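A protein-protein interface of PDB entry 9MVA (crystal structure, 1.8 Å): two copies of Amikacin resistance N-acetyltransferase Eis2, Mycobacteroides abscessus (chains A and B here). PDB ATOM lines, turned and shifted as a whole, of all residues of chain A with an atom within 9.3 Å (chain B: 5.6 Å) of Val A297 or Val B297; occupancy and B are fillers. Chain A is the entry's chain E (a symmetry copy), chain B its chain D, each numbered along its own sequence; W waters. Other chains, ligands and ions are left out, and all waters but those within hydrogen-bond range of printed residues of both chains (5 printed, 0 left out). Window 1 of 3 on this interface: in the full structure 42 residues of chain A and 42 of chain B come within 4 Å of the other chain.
Printed residues of chain B within 4 Å of Glu A135: Arg B284 (2.7 Å). Printed residues of chain B within 4 Å of Arg A284: Glu B135. Printed residues of chain B within 4 Å of His A290: Glu B135 (2.8 Å) and Asp B299 (3.6 Å). Printed residues of chain B within 4 Å of Pro A291: Asp B299 (3.2 Å). Printed residues of chain A within 4 Å of Glu B135: Arg A284 and His A290. Glu B138 touches none of the printed residues of chain A. Of chain A, only Cys A295 (2.9 Å) and Val A297 (3.8 Å) come within 4 Å of Val B297. No residue of chain A comes within 4 Å of Ser B298. The nearest printed residue of chain B that does not touch Pro A291 is Ser B298 (5.0 Å).
His A290 touches Asp B299 (CD2 to CB, 3.6 Å). Pro A291 touches Asp B299 (CB to OD1, 3.2 Å). Val B296 touches Cys A295 (CA to O, 3.6 Å). Val A296 touches Cys B295. Val A297 touches Val B297.
Water W5 bridges OH of Tyr A285 (2.7 Å) and OE2 of Glu B135 (2.7 Å). Water W2 lies within hydrogen-bond range of O of Val B297 and N of Cys A295. Water W4 lies within hydrogen-bond range of the backbone carbonyl oxygen of Val A297 (2.8 Å) and the backbone NH of Cys B295 (3.0 Å). Water W3 lies within hydrogen-bond range of O of Val A297 (3.0 Å), O of Leu B293 (3.1 Å) and NH2 of Arg B284 (3.5 Å). Water W1 bridges O of Val B297 (3.0 Å) and O of Leu A293 (3.1 Å).
The side-chain carboxylate of Glu B135 is in salt-bridge range of the guanidinium group of Arg A284, 2.8 Å away. OE1 of Glu B135 is in hydrogen-bond range of NE2 of His A290 (2.8 Å). The backbone carbonyl oxygen of Cys B295 sits at hydrogen-bond distance from the backbone NH of Val A297. NH2 of Arg B284 is in salt-bridge range of OE1 of Glu A135. The backbone NH of Val B297 is in hydrogen-bond range of the backbone carbonyl oxygen of Cys A295 (2.9 Å).
Of the 13 printed residues of chain B, 6 touch a printed residue of chain A. Printed residues of chain B that touch a printed residue of chain A: Glu B135, Arg B284, Cys B295, Val B296, Val B297 and Asp B299. Among the printed residues, 10 pairs touch across the chains.
N of Glu A138 sits at hydrogen-bond distance from O of Val A296, at 2.8 Å. O of Val B296 is in hydrogen-bond range of N of Glu B138 (2.8 Å). O of Val A279 is in hydrogen-bond range of NH1 of Arg A284. SG of Cys A295 sits at hydrogen-bond distance from NE of Arg A284. The side-chain sulfur (SG) of Cys B295 is in hydrogen-bond range of the guanidinium group (NE) of Arg B284. The backbone carbonyl oxygen of Val B279 sits at hydrogen-bond distance from the guanidinium group of Arg B284 (3.1 Å).
Glu A135 touches Arg B284, and with the chains exchanged Arg A284 touches Glu B135. Cys A295 touches Val B296, and with the chains exchanged Val A296 touches Cys B295. Cys A295 touches Val B297, and with the chains exchanged Val A297 touches Cys B295. Val B297 touches its own counterpart, Val A297. 13 positions are printed for both chains. Of the 10 pairs that touch across the chains among the printed residues, 7 have their exchanged pair printed and touching as well.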
ATOM      1  N   VAL A 132     -33.637  26.965   6.038  1.00  0.00           N
ATOM      2  CA  VAL A 132     -32.572  27.001   7.042  1.00  0.00           C
ATOM      3  C   VAL A 132     -31.973  25.610   7.141  1.00  0.00           C
ATOM      4  O   VAL A 132     -32.666  24.646   7.490  1.00  0.00           O
ATOM      5  CB  VAL A 132     -33.094  27.485   8.398  1.00  0.00           C
ATOM      6  CG1 VAL A 132     -31.971  27.375   9.443  1.00  0.00           C
ATOM      7  CG2 VAL A 132     -33.586  28.941   8.297  1.00  0.00           C
ATOM      8  N   THR A 134     -28.387  25.189   8.336  1.00  0.00           N
ATOM      9  CA  THR A 134     -27.308  25.185   9.308  1.00  0.00           C
ATOM     10  C   THR A 134     -27.676  26.139  10.425  1.00  0.00           C
ATOM     11  O   THR A 134     -28.179  27.236  10.168  1.00  0.00           O
ATOM     12  CB  THR A 134     -25.992  25.615   8.650  1.00  0.00           C
ATOM     13  OG1 THR A 134     -25.705  24.706   7.570  1.00  0.00           O
ATOM     14  CG2 THR A 134     -24.846  25.606   9.659  1.00  0.00           C
ATOM     15  N   GLU A 135     -27.425  25.720  11.661  1.00  0.00           N
ATOM     16  CA  GLU A 135     -27.586  26.586  12.819  1.00  0.00           C
ATOM     17  C   GLU A 135     -26.208  26.965  13.342  1.00  0.00           C
ATOM     18  O   GLU A 135     -25.209  26.315  13.039  1.00  0.00           O
ATOM     19  CB  GLU A 135     -28.405  25.893  13.910  1.00  0.00           C
ATOM     20  CG  GLU A 135     -29.812  25.503  13.438  1.00  0.00           C
ATOM     21  CD  GLU A 135     -30.778  25.325  14.593  1.00  0.00           C
ATOM     22  OE1 GLU A 135     -31.314  26.341  15.104  1.00  0.00           O
ATOM     23  OE2 GLU A 135     -30.992  24.167  15.006  1.00  0.00           O
ATOM     24  N   SER A 136     -26.144  28.039  14.112  1.00  0.00           N
ATOM     25  CA  SER A 136     -24.893  28.350  14.780  1.00  0.00           C
ATOM     26  C   SER A 136     -25.151  28.566  16.260  1.00  0.00           C
ATOM     27  O   SER A 136     -26.291  28.785  16.699  1.00  0.00           O
ATOM     28  CB  SER A 136     -24.196  29.560  14.169  1.00  0.00           C
ATOM     29  OG  SER A 136     -24.969  30.720  14.358  1.00  0.00           O
ATOM     30  N   ALA A 137     -24.068  28.461  17.028  1.00  0.00           N
ATOM     31  CA  ALA A 137     -24.124  28.543  18.478  1.00  0.00           C
ATOM     32  C   ALA A 137     -23.290  29.728  18.935  1.00  0.00           C
ATOM     33  O   ALA A 137     -22.135  29.875  18.521  1.00  0.00           O
ATOM     34  CB  ALA A 137     -23.595  27.252  19.115  1.00  0.00           C
ATOM     35  N   GLU A 138     -23.875  30.586  19.767  1.00  0.00           N
ATOM     36  CA  GLU A 138     -23.074  31.502  20.566  1.00  0.00           C
ATOM     37  C   GLU A 138     -22.678  30.741  21.821  1.00  0.00           C
ATOM     38  O   GLU A 138     -23.551  30.363  22.612  1.00  0.00           O
ATOM     39  CB  GLU A 138     -23.845  32.766  20.922  1.00  0.00           C
ATOM     40  CG  GLU A 138     -23.069  33.627  21.888  1.00  0.00           C
ATOM     41  CD  GLU A 138     -23.942  34.684  22.551  1.00  0.00           C
ATOM     42  OE1 GLU A 138     -24.705  34.359  23.495  1.00  0.00           O
ATOM     43  OE2 GLU A 138     -23.867  35.841  22.111  1.00  0.00           O
ATOM     44  N   LEU A 139     -21.380  30.472  21.981  1.00  0.00           N
ATOM     45  CA  LEU A 139     -20.855  29.769  23.140  1.00  0.00           C
ATOM     46  C   LEU A 139     -20.177  30.782  24.054  1.00  0.00           C
ATOM     47  O   LEU A 139     -19.370  31.592  23.586  1.00  0.00           O
ATOM     48  CB  LEU A 139     -19.856  28.689  22.718  1.00  0.00           C
ATOM     49  CG  LEU A 139     -20.407  27.631  21.758  1.00  0.00           C
ATOM     50  CD1 LEU A 139     -19.279  26.717  21.281  1.00  0.00           C
ATOM     51  CD2 LEU A 139     -21.476  26.817  22.466  1.00  0.00           C
ATOM     52  N   SER A 140     -20.511  30.760  25.343  1.00  0.00           N
ATOM     53  CA  SER A 140     -19.960  31.788  26.217  1.00  0.00           C
ATOM     54  C   SER A 140     -19.913  31.289  27.647  1.00  0.00           C
ATOM     55  O   SER A 140     -20.627  30.360  28.031  1.00  0.00           O
ATOM     56  CB  SER A 140     -20.775  33.088  26.153  1.00  0.00           C
ATOM     57  OG  SER A 140     -22.089  32.896  26.651  1.00  0.00           O
ATOM     58  N   GLY A 276     -21.034  32.414  16.403  1.00  0.00           N
ATOM     59  CA  GLY A 276     -20.975  31.701  15.147  1.00  0.00           C
ATOM     60  C   GLY A 276     -20.368  30.319  15.220  1.00  0.00           C
ATOM     61  O   GLY A 276     -20.062  29.742  14.170  1.00  0.00           O
ATOM     62  N   ALA A 277     -20.204  29.758  16.415  1.00  0.00           N
ATOM     63  CA  ALA A 277     -19.614  28.436  16.556  1.00  0.00           C
ATOM     64  C   ALA A 277     -20.549  27.354  16.011  1.00  0.00           C
ATOM     65  O   ALA A 277     -21.713  27.599  15.682  1.00  0.00           O
ATOM     66  CB  ALA A 277     -19.284  28.165  18.027  1.00  0.00           C
ATOM     67  N   SER A 278     -20.030  26.132  15.924  1.00  0.00           N
ATOM     68  CA  SER A 278     -20.871  24.998  15.559  1.00  0.00           C
ATOM     69  C   SER A 278     -21.706  24.559  16.753  1.00  0.00           C
ATOM     70  O   SER A 278     -21.266  24.647  17.903  1.00  0.00           O
ATOM     71  CB  SER A 278     -20.018  23.817  15.088  1.00  0.00           C
ATOM     72  OG  SER A 278     -20.808  22.639  15.062  1.00  0.00           O
ATOM     73  N   VAL A 279     -22.918  24.067  16.481  1.00  0.00           N
ATOM     74  CA  VAL A 279     -23.710  23.498  17.569  1.00  0.00           C
ATOM     75  C   VAL A 279     -23.099  22.206  18.090  1.00  0.00           C
ATOM     76  O   VAL A 279     -23.530  21.707  19.132  1.00  0.00           O
ATOM     77  CB  VAL A 279     -25.179  23.257  17.160  1.00  0.00           C
ATOM     78  CG1 VAL A 279     -25.824  24.576  16.731  1.00  0.00           C
ATOM     79  CG2 VAL A 279     -25.282  22.205  16.044  1.00  0.00           C
ATOM     80  N   GLN A 280     -22.106  21.658  17.383  1.00  0.00           N
ATOM     81  CA  GLN A 280     -21.317  20.518  17.837  1.00  0.00           C
ATOM     82  C   GLN A 280     -19.839  20.886  17.908  1.00  0.00           C
ATOM     83  O   GLN A 280     -18.964  20.049  17.651  1.00  0.00           O
ATOM     84  CB  GLN A 280     -21.522  19.306  16.925  1.00  0.00           C
ATOM     85  CG  GLN A 280     -22.943  18.758  16.937  1.00  0.00           C
ATOM     86  CD  GLN A 280     -23.093  17.468  16.126  1.00  0.00           C
ATOM     87  OE1 GLN A 280     -22.330  17.195  15.184  1.00  0.00           O
ATOM     88  NE2 GLN A 280     -24.086  16.671  16.490  1.00  0.00           N
ATOM     89  N   ARG A 284     -17.362  22.253  23.165  1.00  0.00           N
ATOM     90  CA  ARG A 284     -18.497  21.917  24.027  1.00  0.00           C
ATOM     91  C   ARG A 284     -18.258  20.628  24.800  1.00  0.00           C
ATOM     92  O   ARG A 284     -18.804  20.449  25.896  1.00  0.00           O
ATOM     93  CB  ARG A 284     -19.772  21.786  23.193  1.00  0.00           C
ATOM     94  CG  ARG A 284     -20.100  23.026  22.348  1.00  0.00           C
ATOM     95  CD  ARG A 284     -21.521  22.929  21.780  1.00  0.00           C
ATOM     96  NE  ARG A 284     -22.500  23.093  22.849  1.00  0.00           N
ATOM     97  CZ  ARG A 284     -23.536  22.297  23.075  1.00  0.00           C
ATOM     98  NH1 ARG A 284     -23.885  21.354  22.216  1.00  0.00           N
ATOM     99  NH2 ARG A 284     -24.237  22.454  24.197  1.00  0.00           N
ATOM    100  N   TYR A 285     -17.465  19.716  24.243  1.00  0.00           N
ATOM    101  CA  TYR A 285     -17.233  18.421  24.868  1.00  0.00           C
ATOM    102  C   TYR A 285     -15.905  18.352  25.604  1.00  0.00           C
ATOM    103  O   TYR A 285     -15.716  17.451  26.431  1.00  0.00           O
ATOM    104  CB  TYR A 285     -17.327  17.305  23.808  1.00  0.00           C
ATOM    105  CG  TYR A 285     -18.609  17.464  23.031  1.00  0.00           C
ATOM    106  CD1 TYR A 285     -19.826  17.084  23.592  1.00  0.00           C
ATOM    107  CD2 TYR A 285     -18.621  18.089  21.788  1.00  0.00           C
ATOM    108  CE1 TYR A 285     -21.018  17.272  22.918  1.00  0.00           C
ATOM    109  CE2 TYR A 285     -19.810  18.280  21.098  1.00  0.00           C
ATOM    110  CZ  TYR A 285     -21.006  17.876  21.673  1.00  0.00           C
ATOM    111  OH  TYR A 285     -22.195  18.066  20.996  1.00  0.00           O
ATOM    112  N   HIS A 290     -20.190  20.556  31.467  1.00  0.00           N
ATOM    113  CA  HIS A 290     -20.930  20.867  30.244  1.00  0.00           C
ATOM    114  C   HIS A 290     -21.664  22.204  30.293  1.00  0.00           C
ATOM    115  O   HIS A 290     -21.421  23.037  29.408  1.00  0.00           O
ATOM    116  CB  HIS A 290     -21.856  19.666  29.987  1.00  0.00           C
ATOM    117  CG  HIS A 290     -22.666  19.755  28.728  1.00  0.00           C
ATOM    118  ND1 HIS A 290     -22.616  18.782  27.755  1.00  0.00           N
ATOM    119  CD2 HIS A 290     -23.589  20.657  28.312  1.00  0.00           C
ATOM    120  CE1 HIS A 290     -23.446  19.098  26.774  1.00  0.00           C
ATOM    121  NE2 HIS A 290     -24.053  20.227  27.091  1.00  0.00           N
ATOM    122  N   PRO A 291     -22.522  22.499  31.281  1.00  0.00           N
ATOM    123  CA  PRO A 291     -23.299  23.754  31.220  1.00  0.00           C
ATOM    124  C   PRO A 291     -22.499  25.010  31.513  1.00  0.00           C
ATOM    125  O   PRO A 291     -23.035  26.106  31.313  1.00  0.00           O
ATOM    126  CB  PRO A 291     -24.391  23.552  32.281  1.00  0.00           C
ATOM    127  CG  PRO A 291     -23.754  22.629  33.274  1.00  0.00           C
ATOM    128  CD  PRO A 291     -22.944  21.669  32.423  1.00  0.00           C
ATOM    129  N   SER A 292     -21.258  24.909  32.000  1.00  0.00           N
ATOM    130  CA  SER A 292     -20.464  26.120  32.159  1.00  0.00           C
ATOM    131  C   SER A 292     -20.262  26.847  30.835  1.00  0.00           C
ATOM    132  O   SER A 292     -20.037  28.061  30.830  1.00  0.00           O
ATOM    133  CB  SER A 292     -19.111  25.788  32.792  1.00  0.00           C
ATOM    134  OG  SER A 292     -19.308  25.358  34.126  1.00  0.00           O
ATOM    135  N   LEU A 293     -20.351  26.140  29.708  1.00  0.00           N
ATOM    136  CA  LEU A 293     -20.270  26.765  28.392  1.00  0.00           C
ATOM    137  C   LEU A 293     -21.701  26.961  27.897  1.00  0.00           C
ATOM    138  O   LEU A 293     -22.311  26.039  27.352  1.00  0.00           O
ATOM    139  CB  LEU A 293     -19.441  25.906  27.437  1.00  0.00           C
ATOM    140  CG  LEU A 293     -19.111  26.603  26.114  1.00  0.00           C
ATOM    141  CD1 LEU A 293     -18.273  27.878  26.333  1.00  0.00           C
ATOM    142  CD2 LEU A 293     -18.409  25.638  25.172  1.00  0.00           C
ATOM    143  N   GLU A 294     -22.253  28.157  28.121  1.00  0.00           N
ATOM    144  CA  GLU A 294     -23.618  28.436  27.706  1.00  0.00           C
ATOM    145  C   GLU A 294     -23.714  28.370  26.192  1.00  0.00           C
ATOM    146  O   GLU A 294     -22.743  28.641  25.484  1.00  0.00           O
ATOM    147  CB  GLU A 294     -24.048  29.815  28.199  1.00  0.00           C
ATOM    148  CG  GLU A 294     -23.953  29.952  29.717  1.00  0.00           C
ATOM    149  CD  GLU A 294     -24.515  31.273  30.188  1.00  0.00           C
ATOM    150  OE1 GLU A 294     -25.426  31.798  29.529  1.00  0.00           O
ATOM    151  OE2 GLU A 294     -24.049  31.783  31.214  1.00  0.00           O
ATOM    152  N   CYS A 295     -24.890  27.977  25.691  1.00  0.00           N
ATOM    153  CA  CYS A 295     -25.041  27.631  24.275  1.00  0.00           C
ATOM    154  C   CYS A 295     -26.376  28.172  23.788  1.00  0.00           C
ATOM    155  O   CYS A 295     -27.424  27.635  24.147  1.00  0.00           O
ATOM    156  CB  CYS A 295     -24.982  26.118  24.056  1.00  0.00           C
ATOM    157  SG  CYS A 295     -25.084  25.619  22.285  1.00  0.00           S
ATOM    158  N   VAL A 296     -26.340  29.215  22.967  1.00  0.00           N
ATOM    159  CA  VAL A 296     -27.544  29.823  22.404  1.00  0.00           C
ATOM    160  C   VAL A 296     -27.531  29.584  20.906  1.00  0.00           C
ATOM    161  O   VAL A 296     -26.562  29.945  20.225  1.00  0.00           O
ATOM    162  CB  VAL A 296     -27.616  31.322  22.719  1.00  0.00           C
ATOM    163  CG1 VAL A 296     -28.856  31.959  22.040  1.00  0.00           C
ATOM    164  CG2 VAL A 296     -27.642  31.526  24.221  1.00  0.00           C
ATOM    165  N   VAL A 297     -28.612  28.995  20.392  1.00  0.00           N
ATOM    166  CA  VAL A 297     -28.645  28.424  19.046  1.00  0.00           C
ATOM    167  C   VAL A 297     -29.632  29.222  18.204  1.00  0.00           C
ATOM    168  O   VAL A 297     -30.760  29.475  18.644  1.00  0.00           O
ATOM    169  CB  VAL A 297     -29.047  26.938  19.080  1.00  0.00           C
ATOM    170  CG1 VAL A 297     -29.161  26.383  17.672  1.00  0.00           C
ATOM    171  CG2 VAL A 297     -28.027  26.128  19.883  1.00  0.00           C
ATOM    172  N   SER A 298     -29.209  29.619  17.005  1.00  0.00           N
ATOM    173  CA  SER A 298     -30.109  30.260  16.053  1.00  0.00           C
ATOM    174  C   SER A 298     -29.769  29.814  14.639  1.00  0.00           C
ATOM    175  O   SER A 298     -28.795  29.103  14.399  1.00  0.00           O
ATOM    176  CB  SER A 298     -30.042  31.789  16.149  1.00  0.00           C
ATOM    177  OG  SER A 298     -28.700  32.219  15.999  1.00  0.00           O
ATOM    178  N   ASP A 299     -30.596  30.265  13.698  1.00  0.00           N
ATOM    179  CA  ASP A 299     -30.386  29.973  12.285  1.00  0.00           C
ATOM    180  C   ASP A 299     -29.092  30.603  11.783  1.00  0.00           C
ATOM    181  O   ASP A 299     -28.722  31.712  12.183  1.00  0.00           O
ATOM    182  CB  ASP A 299     -31.576  30.502  11.477  1.00  0.00           C
ATOM    183  CG  ASP A 299     -31.791  31.990  11.672  1.00  0.00           C
ATOM    184  OD1 ASP A 299     -31.971  32.453  12.823  1.00  0.00           O
ATOM    185  OD2 ASP A 299     -31.742  32.719  10.675  1.00  0.00           O
ATOM    186  N   ALA A 300     -28.390  29.886  10.906  1.00  0.00           N
ATOM    187  CA  ALA A 300     -27.187  30.430  10.289  1.00  0.00           C
ATOM    188  C   ALA A 300     -27.384  30.528   8.779  1.00  0.00           C
ATOM    189  O   ALA A 300     -27.803  31.577   8.280  1.00  0.00           O
ATOM    190  CB  ALA A 300     -25.953  29.584  10.630  1.00  0.00           C
ATOM    191  N   GLY A 373     -28.048  19.171   8.868  1.00  0.00           N
ATOM    192  CA  GLY A 373     -28.245  19.954  10.083  1.00  0.00           C
ATOM    193  C   GLY A 373     -29.670  19.974  10.600  1.00  0.00           C
ATOM    194  O   GLY A 373     -29.933  20.468  11.703  1.00  0.00           O
ATOM    195  N   GLU B 135     -29.371  16.418  25.582  1.00  0.00           N
ATOM    196  CA  GLU B 135     -29.438  17.837  25.888  1.00  0.00           C
ATOM    197  C   GLU B 135     -30.891  18.259  25.863  1.00  0.00           C
ATOM    198  O   GLU B 135     -31.753  17.553  25.335  1.00  0.00           O
ATOM    199  CB  GLU B 135     -28.619  18.679  24.900  1.00  0.00           C
ATOM    200  CG  GLU B 135     -27.113  18.338  24.930  1.00  0.00           C
ATOM    201  CD  GLU B 135     -26.246  19.462  24.357  1.00  0.00           C
ATOM    202  OE1 GLU B 135     -25.970  20.451  25.074  1.00  0.00           O
ATOM    203  OE2 GLU B 135     -25.863  19.384  23.178  1.00  0.00           O
ATOM    204  N   SER B 136     -31.169  19.412  26.453  1.00  0.00           N
ATOM    205  CA  SER B 136     -32.511  19.957  26.383  1.00  0.00           C
ATOM    206  C   SER B 136     -32.450  21.409  25.939  1.00  0.00           C
ATOM    207  O   SER B 136     -31.411  22.076  26.023  1.00  0.00           O
ATOM    208  CB  SER B 136     -33.243  19.834  27.719  1.00  0.00           C
ATOM    209  OG  SER B 136     -32.533  20.517  28.720  1.00  0.00           O
ATOM    210  N   ALA B 137     -33.589  21.885  25.449  1.00  0.00           N
ATOM    211  CA  ALA B 137     -33.717  23.235  24.930  1.00  0.00           C
ATOM    212  C   ALA B 137     -34.760  23.972  25.748  1.00  0.00           C
ATOM    213  O   ALA B 137     -35.857  23.452  25.971  1.00  0.00           O
ATOM    214  CB  ALA B 137     -34.129  23.222  23.452  1.00  0.00           C
ATOM    215  N   GLU B 138     -34.410  25.163  26.215  1.00  0.00           N
ATOM    216  CA  GLU B 138     -35.406  26.131  26.659  1.00  0.00           C
ATOM    217  C   GLU B 138     -35.793  26.942  25.436  1.00  0.00           C
ATOM    218  O   GLU B 138     -34.961  27.668  24.882  1.00  0.00           O
ATOM    219  CB  GLU B 138     -34.856  27.033  27.760  1.00  0.00           C
ATOM    220  CG  GLU B 138     -35.762  28.222  28.032  1.00  0.00           C
ATOM    221  CD  GLU B 138     -35.074  29.335  28.821  1.00  0.00           C
ATOM    222  OE1 GLU B 138     -34.894  29.153  30.044  1.00  0.00           O
ATOM    223  OE2 GLU B 138     -34.713  30.380  28.216  1.00  0.00           O
ATOM    224  N   VAL B 279     -34.080  19.480  21.617  1.00  0.00           N
ATOM    225  CA  VAL B 279     -33.282  20.327  20.733  1.00  0.00           C
ATOM    226  C   VAL B 279     -33.747  20.223  19.288  1.00  0.00           C
ATOM    227  O   VAL B 279     -33.370  21.059  18.456  1.00  0.00           O
ATOM    228  CB  VAL B 279     -31.776  19.990  20.838  1.00  0.00           C
ATOM    229  CG1 VAL B 279     -31.301  20.188  22.269  1.00  0.00           C
ATOM    230  CG2 VAL B 279     -31.471  18.552  20.371  1.00  0.00           C
ATOM    231  N   ARG B 284     -39.869  23.982  16.616  1.00  0.00           N
ATOM    232  CA  ARG B 284     -38.780  24.802  16.084  1.00  0.00           C
ATOM    233  C   ARG B 284     -38.887  24.977  14.575  1.00  0.00           C
ATOM    234  O   ARG B 284     -38.438  25.994  14.036  1.00  0.00           O
ATOM    235  CB  ARG B 284     -37.429  24.171  16.431  1.00  0.00           C
ATOM    236  CG  ARG B 284     -37.213  23.976  17.928  1.00  0.00           C
ATOM    237  CD  ARG B 284     -35.737  23.639  18.246  1.00  0.00           C
ATOM    238  NE  ARG B 284     -34.902  24.810  18.019  1.00  0.00           N
ATOM    239  CZ  ARG B 284     -33.788  24.844  17.307  1.00  0.00           C
ATOM    240  NH1 ARG B 284     -33.221  23.734  16.852  1.00  0.00           N
ATOM    241  NH2 ARG B 284     -33.219  26.022  17.049  1.00  0.00           N
ATOM    242  N   LEU B 293     -38.216  31.905  17.778  1.00  0.00           N
ATOM    243  CA  LEU B 293     -38.241  30.967  18.891  1.00  0.00           C
ATOM    244  C   LEU B 293     -36.802  30.840  19.371  1.00  0.00           C
ATOM    245  O   LEU B 293     -36.004  30.098  18.787  1.00  0.00           O
ATOM    246  CB  LEU B 293     -38.826  29.624  18.465  1.00  0.00           C
ATOM    247  CG  LEU B 293     -39.180  28.668  19.611  1.00  0.00           C
ATOM    248  CD1 LEU B 293     -40.321  29.253  20.459  1.00  0.00           C
ATOM    249  CD2 LEU B 293     -39.538  27.286  19.073  1.00  0.00           C
ATOM    250  N   GLU B 294     -36.458  31.601  20.408  1.00  0.00           N
ATOM    251  CA  GLU B 294     -35.121  31.499  20.979  1.00  0.00           C
ATOM    252  C   GLU B 294     -34.893  30.103  21.539  1.00  0.00           C
ATOM    253  O   GLU B 294     -35.821  29.441  22.012  1.00  0.00           O
ATOM    254  CB  GLU B 294     -34.935  32.541  22.077  1.00  0.00           C
ATOM    255  CG  GLU B 294     -35.232  33.944  21.594  1.00  0.00           C
ATOM    256  CD  GLU B 294     -34.883  34.983  22.642  1.00  0.00           C
ATOM    257  OE1 GLU B 294     -33.960  34.739  23.439  1.00  0.00           O
ATOM    258  OE2 GLU B 294     -35.534  36.033  22.676  1.00  0.00           O
ATOM    259  N   CYS B 295     -33.632  29.662  21.496  1.00  0.00           N
ATOM    260  CA  CYS B 295     -33.264  28.289  21.830  1.00  0.00           C
ATOM    261  C   CYS B 295     -31.988  28.312  22.664  1.00  0.00           C
ATOM    262  O   CYS B 295     -30.919  28.653  22.151  1.00  0.00           O
ATOM    263  CB  CYS B 295     -33.054  27.460  20.564  1.00  0.00           C
ATOM    264  SG  CYS B 295     -32.694  25.727  20.890  1.00  0.00           S
ATOM    265  N   VAL B 296     -32.095  27.945  23.938  1.00  0.00           N
ATOM    266  CA  VAL B 296     -30.955  27.858  24.846  1.00  0.00           C
ATOM    267  C   VAL B 296     -30.763  26.391  25.205  1.00  0.00           C
ATOM    268  O   VAL B 296     -31.703  25.735  25.671  1.00  0.00           O
ATOM    269  CB  VAL B 296     -31.169  28.711  26.108  1.00  0.00           C
ATOM    270  CG1 VAL B 296     -29.966  28.551  27.064  1.00  0.00           C
ATOM    271  CG2 VAL B 296     -31.345  30.178  25.731  1.00  0.00           C
ATOM    272  N   VAL B 297     -29.559  25.872  24.984  1.00  0.00           N
ATOM    273  CA  VAL B 297     -29.309  24.432  25.035  1.00  0.00           C
ATOM    274  C   VAL B 297     -28.384  24.114  26.203  1.00  0.00           C
ATOM    275  O   VAL B 297     -27.358  24.779  26.396  1.00  0.00           O
ATOM    276  CB  VAL B 297     -28.723  23.918  23.708  1.00  0.00           C
ATOM    277  CG1 VAL B 297     -28.369  22.451  23.813  1.00  0.00           C
ATOM    278  CG2 VAL B 297     -29.740  24.113  22.591  1.00  0.00           C
ATOM    279  N   SER B 298     -28.746  23.095  26.980  1.00  0.00           N
ATOM    280  CA  SER B 298     -27.940  22.691  28.119  1.00  0.00           C
ATOM    281  C   SER B 298     -27.973  21.174  28.267  1.00  0.00           C
ATOM    282  O   SER B 298     -28.696  20.462  27.565  1.00  0.00           O
ATOM    283  CB  SER B 298     -28.424  23.375  29.407  1.00  0.00           C
ATOM    284  OG  SER B 298     -29.743  22.969  29.728  1.00  0.00           O
ATOM    285  N   ASP B 299     -27.166  20.673  29.198  1.00  0.00           N
ATOM    286  CA  ASP B 299     -27.140  19.241  29.444  1.00  0.00           C
ATOM    287  C   ASP B 299     -28.448  18.787  30.070  1.00  0.00           C
ATOM    288  O   ASP B 299     -29.075  19.507  30.847  1.00  0.00           O
ATOM    289  CB  ASP B 299     -25.981  18.879  30.370  1.00  0.00           C
ATOM    290  CG  ASP B 299     -26.027  19.656  31.651  1.00  0.00           C
ATOM    291  OD1 ASP B 299     -26.061  20.913  31.588  1.00  0.00           O
ATOM    292  OD2 ASP B 299     -26.092  19.021  32.719  1.00  0.00           O
HETATM  293  O   HOH W   1     -24.638  23.971  27.409  1.00  0.00           O
HETATM  294  O   HOH W   2     -26.660  27.058  27.819  1.00  0.00           O
HETATM  295  O   HOH W   3     -33.393  29.493  17.304  1.00  0.00           O
HETATM  296  O   HOH W   4     -31.885  31.604  20.059  1.00  0.00           O
HETATM  297  O   HOH W   5     -24.473  17.309  22.128  1.00  0.00           O
